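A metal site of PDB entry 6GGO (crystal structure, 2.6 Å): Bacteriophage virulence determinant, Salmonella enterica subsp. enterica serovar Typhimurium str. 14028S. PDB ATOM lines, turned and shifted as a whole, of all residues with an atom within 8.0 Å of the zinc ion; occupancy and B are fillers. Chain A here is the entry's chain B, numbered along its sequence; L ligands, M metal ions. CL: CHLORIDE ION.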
ATOM      1  N   PHE A 115     -13.792 -27.321 -14.054  1.00  0.00           N
ATOM      2  CA  PHE A 115     -14.310 -26.963 -12.740  1.00  0.00           C
ATOM      3  C   PHE A 115     -13.909 -25.549 -12.367  1.00  0.00           C
ATOM      4  O   PHE A 115     -12.718 -25.198 -12.400  1.00  0.00           O
ATOM      5  CB  PHE A 115     -13.812 -27.943 -11.680  1.00  0.00           C
ATOM      6  CG  PHE A 115     -14.485 -29.284 -11.726  1.00  0.00           C
ATOM      7  CD1 PHE A 115     -15.800 -29.414 -11.321  1.00  0.00           C
ATOM      8  CD2 PHE A 115     -13.797 -30.411 -12.145  1.00  0.00           C
ATOM      9  CE1 PHE A 115     -16.426 -30.649 -11.349  1.00  0.00           C
ATOM     10  CE2 PHE A 115     -14.415 -31.640 -12.170  1.00  0.00           C
ATOM     11  CZ  PHE A 115     -15.736 -31.762 -11.768  1.00  0.00           C
ATOM     12  N   GLY A 116     -14.889 -24.741 -12.000  1.00  0.00           N
ATOM     13  CA  GLY A 116     -14.625 -23.382 -11.590  1.00  0.00           C
ATOM     14  C   GLY A 116     -15.913 -22.663 -11.284  1.00  0.00           C
ATOM     15  O   GLY A 116     -17.001 -23.065 -11.723  1.00  0.00           O
ATOM     16  N   THR A 117     -15.789 -21.588 -10.511  1.00  0.00           N
ATOM     17  CA  THR A 117     -16.926 -20.779 -10.088  1.00  0.00           C
ATOM     18  C   THR A 117     -16.502 -19.330 -10.045  1.00  0.00           C
ATOM     19  O   THR A 117     -15.468 -18.994  -9.458  1.00  0.00           O
ATOM     20  CB  THR A 117     -17.444 -21.218  -8.714  1.00  0.00           C
ATOM     21  OG1 THR A 117     -17.756 -22.620  -8.738  1.00  0.00           O
ATOM     22  CG2 THR A 117     -18.700 -20.434  -8.336  1.00  0.00           C
ATOM     23  N   VAL A 119     -16.282 -16.180  -8.592  1.00  0.00           N
ATOM     24  CA  VAL A 119     -16.455 -15.502  -7.313  1.00  0.00           C
ATOM     25  C   VAL A 119     -15.595 -14.254  -7.183  1.00  0.00           C
ATOM     26  O   VAL A 119     -15.849 -13.439  -6.286  1.00  0.00           O
ATOM     27  CB  VAL A 119     -16.173 -16.460  -6.137  1.00  0.00           C
ATOM     28  CG1 VAL A 119     -16.867 -17.799  -6.354  1.00  0.00           C
ATOM     29  CG2 VAL A 119     -14.667 -16.650  -5.923  1.00  0.00           C
ATOM     30  N   SER A 163     -15.825 -32.874  -6.004  1.00  0.00           N
ATOM     31  CA  SER A 163     -15.648 -31.853  -7.024  1.00  0.00           C
ATOM     32  C   SER A 163     -16.865 -30.944  -7.098  1.00  0.00           C
ATOM     33  O   SER A 163     -16.743 -29.710  -7.068  1.00  0.00           O
ATOM     34  CB  SER A 163     -15.379 -32.502  -8.386  1.00  0.00           C
ATOM     35  OG  SER A 163     -14.297 -33.416  -8.311  1.00  0.00           O
ATOM     36  N   HIS A 166     -17.415 -28.839  -3.887  1.00  0.00           N
ATOM     37  CA  HIS A 166     -16.435 -27.763  -3.799  1.00  0.00           C
ATOM     38  C   HIS A 166     -16.904 -26.540  -4.579  1.00  0.00           C
ATOM     39  O   HIS A 166     -16.985 -25.427  -4.023  1.00  0.00           O
ATOM     40  CB  HIS A 166     -15.071 -28.240  -4.305  1.00  0.00           C
ATOM     41  CG  HIS A 166     -13.989 -27.224  -4.137  1.00  0.00           C
ATOM     42  ND1 HIS A 166     -13.270 -27.077  -2.964  1.00  0.00           N
ATOM     43  CD2 HIS A 166     -13.492 -26.288  -4.997  1.00  0.00           C
ATOM     44  CE1 HIS A 166     -12.393 -26.105  -3.112  1.00  0.00           C
ATOM     45  NE2 HIS A 166     -12.502 -25.615  -4.333  1.00  0.00           N
ATOM     46  N   GLN A 167     -17.235 -26.725  -5.852  1.00  0.00           N
ATOM     47  CA  GLN A 167     -17.667 -25.591  -6.674  1.00  0.00           C
ATOM     48  C   GLN A 167     -18.966 -24.991  -6.165  1.00  0.00           C
ATOM     49  O   GLN A 167     -19.172 -23.777  -6.276  1.00  0.00           O
ATOM     50  CB  GLN A 167     -17.814 -26.031  -8.128  1.00  0.00           C
ATOM     51  CG  GLN A 167     -16.526 -26.557  -8.757  1.00  0.00           C
ATOM     52  CD  GLN A 167     -15.364 -25.603  -8.626  1.00  0.00           C
ATOM     53  OE1 GLN A 167     -15.548 -24.378  -8.599  1.00  0.00           O
ATOM     54  NE2 GLN A 167     -14.152 -26.140  -8.549  1.00  0.00           N
ATOM     55  N   HIS A 170     -18.304 -22.652  -3.335  1.00  0.00           N
ATOM     56  CA  HIS A 170     -17.857 -21.382  -3.903  1.00  0.00           C
ATOM     57  C   HIS A 170     -19.044 -20.476  -4.214  1.00  0.00           C
ATOM     58  O   HIS A 170     -19.028 -19.279  -3.898  1.00  0.00           O
ATOM     59  CB  HIS A 170     -17.036 -21.635  -5.171  1.00  0.00           C
ATOM     60  CG  HIS A 170     -15.582 -21.892  -4.927  1.00  0.00           C
ATOM     61  ND1 HIS A 170     -14.749 -20.959  -4.364  1.00  0.00           N
ATOM     62  CD2 HIS A 170     -14.812 -22.978  -5.188  1.00  0.00           C
ATOM     63  CE1 HIS A 170     -13.528 -21.455  -4.287  1.00  0.00           C
ATOM     64  NE2 HIS A 170     -13.542 -22.683  -4.772  1.00  0.00           N
ATOM     65  N   LEU A 175     -16.829 -17.288  -1.454  1.00  0.00           N
ATOM     66  CA  LEU A 175     -15.482 -17.315  -0.909  1.00  0.00           C
ATOM     67  C   LEU A 175     -14.524 -18.002  -1.882  1.00  0.00           C
ATOM     68  O   LEU A 175     -14.916 -18.799  -2.726  1.00  0.00           O
ATOM     69  CB  LEU A 175     -15.461 -18.052   0.442  1.00  0.00           C
ATOM     70  CG  LEU A 175     -16.309 -17.446   1.555  1.00  0.00           C
ATOM     71  CD1 LEU A 175     -16.433 -18.413   2.720  1.00  0.00           C
ATOM     72  CD2 LEU A 175     -15.692 -16.131   2.014  1.00  0.00           C
ATOM     73  N   GLN A 176     -13.245 -17.661  -1.738  1.00  0.00           N
ATOM     74  CA  GLN A 176     -12.193 -18.230  -2.555  1.00  0.00           C
ATOM     75  C   GLN A 176     -11.348 -19.168  -1.718  1.00  0.00           C
ATOM     76  O   GLN A 176     -11.430 -19.187  -0.482  1.00  0.00           O
ATOM     77  CB  GLN A 176     -11.320 -17.116  -3.174  1.00  0.00           C
ATOM     78  CG  GLN A 176     -10.977 -15.994  -2.210  1.00  0.00           C
ATOM     79  CD  GLN A 176     -10.312 -14.805  -2.888  1.00  0.00           C
ATOM     80  OE1 GLN A 176     -10.613 -13.652  -2.587  1.00  0.00           O
ATOM     81  NE2 GLN A 176      -9.403 -15.095  -3.813  1.00  0.00           N
ATOM     82  N   ASP A 177     -10.534 -19.986  -2.400  1.00  0.00           N
ATOM     83  CA  ASP A 177      -9.775 -21.022  -1.706  1.00  0.00           C
ATOM     84  C   ASP A 177      -8.565 -20.464  -0.973  1.00  0.00           C
ATOM     85  O   ASP A 177      -8.205 -20.969   0.090  1.00  0.00           O
ATOM     86  CB  ASP A 177      -9.329 -22.086  -2.705  1.00  0.00           C
ATOM     87  CG  ASP A 177     -10.496 -22.834  -3.325  1.00  0.00           C
ATOM     88  OD1 ASP A 177     -11.301 -23.403  -2.562  1.00  0.00           O
ATOM     89  OD2 ASP A 177     -10.604 -22.845  -4.569  1.00  0.00           O
ATOM     90  N   LYS A 178      -7.916 -19.429  -1.512  1.00  0.00           N
ATOM     91  CA  LYS A 178      -6.688 -18.926  -0.907  1.00  0.00           C
ATOM     92  C   LYS A 178      -7.032 -18.022   0.269  1.00  0.00           C
ATOM     93  O   LYS A 178      -7.723 -17.017   0.115  1.00  0.00           O
ATOM     94  CB  LYS A 178      -5.834 -18.183  -1.950  1.00  0.00           C
ATOM     95  CG  LYS A 178      -5.233 -19.130  -2.975  1.00  0.00           C
ATOM     96  CD  LYS A 178      -4.514 -18.393  -4.093  1.00  0.00           C
ATOM     97  CE  LYS A 178      -4.086 -19.366  -5.186  1.00  0.00           C
ATOM     98  NZ  LYS A 178      -3.185 -20.436  -4.658  1.00  0.00           N
ATOM     99  N   ARG A 184      -5.831 -24.618   3.913  1.00  0.00           N
ATOM    100  CA  ARG A 184      -6.969 -25.149   3.174  1.00  0.00           C
ATOM    101  C   ARG A 184      -7.865 -24.073   2.583  1.00  0.00           C
ATOM    102  O   ARG A 184      -8.289 -24.200   1.429  1.00  0.00           O
ATOM    103  CB  ARG A 184      -7.811 -26.042   4.075  1.00  0.00           C
ATOM    104  CG  ARG A 184      -7.138 -27.330   4.489  1.00  0.00           C
ATOM    105  CD  ARG A 184      -7.886 -28.003   5.633  1.00  0.00           C
ATOM    106  NE  ARG A 184      -7.836 -27.202   6.859  1.00  0.00           N
ATOM    107  CZ  ARG A 184      -6.831 -27.212   7.719  1.00  0.00           C
ATOM    108  NH1 ARG A 184      -5.766 -27.966   7.511  1.00  0.00           N
ATOM    109  NH2 ARG A 184      -6.888 -26.447   8.809  1.00  0.00           N
ATOM    110  N   VAL A 187     -13.443 -22.880   1.753  1.00  0.00           N
ATOM    111  CA  VAL A 187     -14.234 -23.739   0.873  1.00  0.00           C
ATOM    112  C   VAL A 187     -13.899 -25.198   1.105  1.00  0.00           C
ATOM    113  O   VAL A 187     -14.792 -26.052   1.244  1.00  0.00           O
ATOM    114  CB  VAL A 187     -14.009 -23.335  -0.605  1.00  0.00           C
ATOM    115  CG1 VAL A 187     -14.752 -24.278  -1.532  1.00  0.00           C
ATOM    116  CG2 VAL A 187     -14.445 -21.903  -0.819  1.00  0.00           C
ATOM    117  N   VAL A 188     -12.604 -25.530   1.151  1.00  0.00           N
ATOM    118  CA  VAL A 188     -12.199 -26.911   1.391  1.00  0.00           C
ATOM    119  C   VAL A 188     -12.773 -27.411   2.717  1.00  0.00           C
ATOM    120  O   VAL A 188     -13.308 -28.521   2.800  1.00  0.00           O
ATOM    121  CB  VAL A 188     -10.660 -27.031   1.362  1.00  0.00           C
ATOM    122  CG1 VAL A 188     -10.208 -28.391   1.869  1.00  0.00           C
ATOM    123  CG2 VAL A 188     -10.139 -26.782  -0.045  1.00  0.00           C
ATOM    124  N   THR A 191     -16.359 -28.023   2.431  1.00  0.00           N
ATOM    125  CA  THR A 191     -16.492 -29.256   1.671  1.00  0.00           C
ATOM    126  C   THR A 191     -16.223 -30.476   2.554  1.00  0.00           C
ATOM    127  O   THR A 191     -16.977 -31.450   2.524  1.00  0.00           O
ATOM    128  CB  THR A 191     -15.542 -29.240   0.481  1.00  0.00           C
ATOM    129  OG1 THR A 191     -15.754 -28.061  -0.300  1.00  0.00           O
ATOM    130  CG2 THR A 191     -15.780 -30.465  -0.398  1.00  0.00           C
ATOM    131  N   ARG A 205      -9.499 -33.364   3.100  1.00  0.00           N
ATOM    132  CA  ARG A 205      -8.451 -32.676   2.346  1.00  0.00           C
ATOM    133  C   ARG A 205      -7.702 -31.756   3.300  1.00  0.00           C
ATOM    134  O   ARG A 205      -8.277 -30.777   3.802  1.00  0.00           O
ATOM    135  CB  ARG A 205      -9.079 -31.914   1.181  1.00  0.00           C
ATOM    136  CG  ARG A 205      -8.133 -31.190   0.242  1.00  0.00           C
ATOM    137  CD  ARG A 205      -8.939 -30.569  -0.893  1.00  0.00           C
ATOM    138  NE  ARG A 205      -8.129 -29.851  -1.865  1.00  0.00           N
ATOM    139  CZ  ARG A 205      -8.618 -29.185  -2.910  1.00  0.00           C
ATOM    140  NH1 ARG A 205      -9.930 -29.134  -3.119  1.00  0.00           N
ATOM    141  NH2 ARG A 205      -7.803 -28.561  -3.741  1.00  0.00           N
ATOM    142  N   TYR A 208      -4.965 -27.198   0.391  1.00  0.00           N
ATOM    143  CA  TYR A 208      -5.423 -26.825  -0.936  1.00  0.00           C
ATOM    144  C   TYR A 208      -4.432 -27.274  -2.007  1.00  0.00           C
ATOM    145  O   TYR A 208      -4.812 -27.959  -2.967  1.00  0.00           O
ATOM    146  CB  TYR A 208      -5.652 -25.316  -1.022  1.00  0.00           C
ATOM    147  CG  TYR A 208      -6.165 -24.873  -2.368  1.00  0.00           C
ATOM    148  CD1 TYR A 208      -7.430 -25.256  -2.805  1.00  0.00           C
ATOM    149  CD2 TYR A 208      -5.395 -24.071  -3.202  1.00  0.00           C
ATOM    150  CE1 TYR A 208      -7.914 -24.854  -4.038  1.00  0.00           C
ATOM    151  CE2 TYR A 208      -5.868 -23.665  -4.441  1.00  0.00           C
ATOM    152  CZ  TYR A 208      -7.131 -24.063  -4.854  1.00  0.00           C
ATOM    153  OH  TYR A 208      -7.610 -23.670  -6.084  1.00  0.00           O
HETATM  154 CL    CL L   1     -10.812 -25.134  -7.958  1.00  0.00          CL
HETATM  155 ZN    ZN M   1     -11.806 -23.973  -5.510  1.00  0.00          ZN
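OD2 of Asp 177 lies close to OH of Tyr 208 (3.5 Å). The backbone carbonyl oxygen (O) of Leu 175 lies within hydrogen-bond range of a ring nitrogen (ND1) of His 170, at 2.7 Å.
Along chain A the residues within 4 Å of the zinc ion span positions 166 to 177.
The zinc ion is bound by OD2 of Asp 177, NE2 of His 166 and NE2 of His 170. Slightly farther from the zinc ion lies CL of the ligand (2.9 Å).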
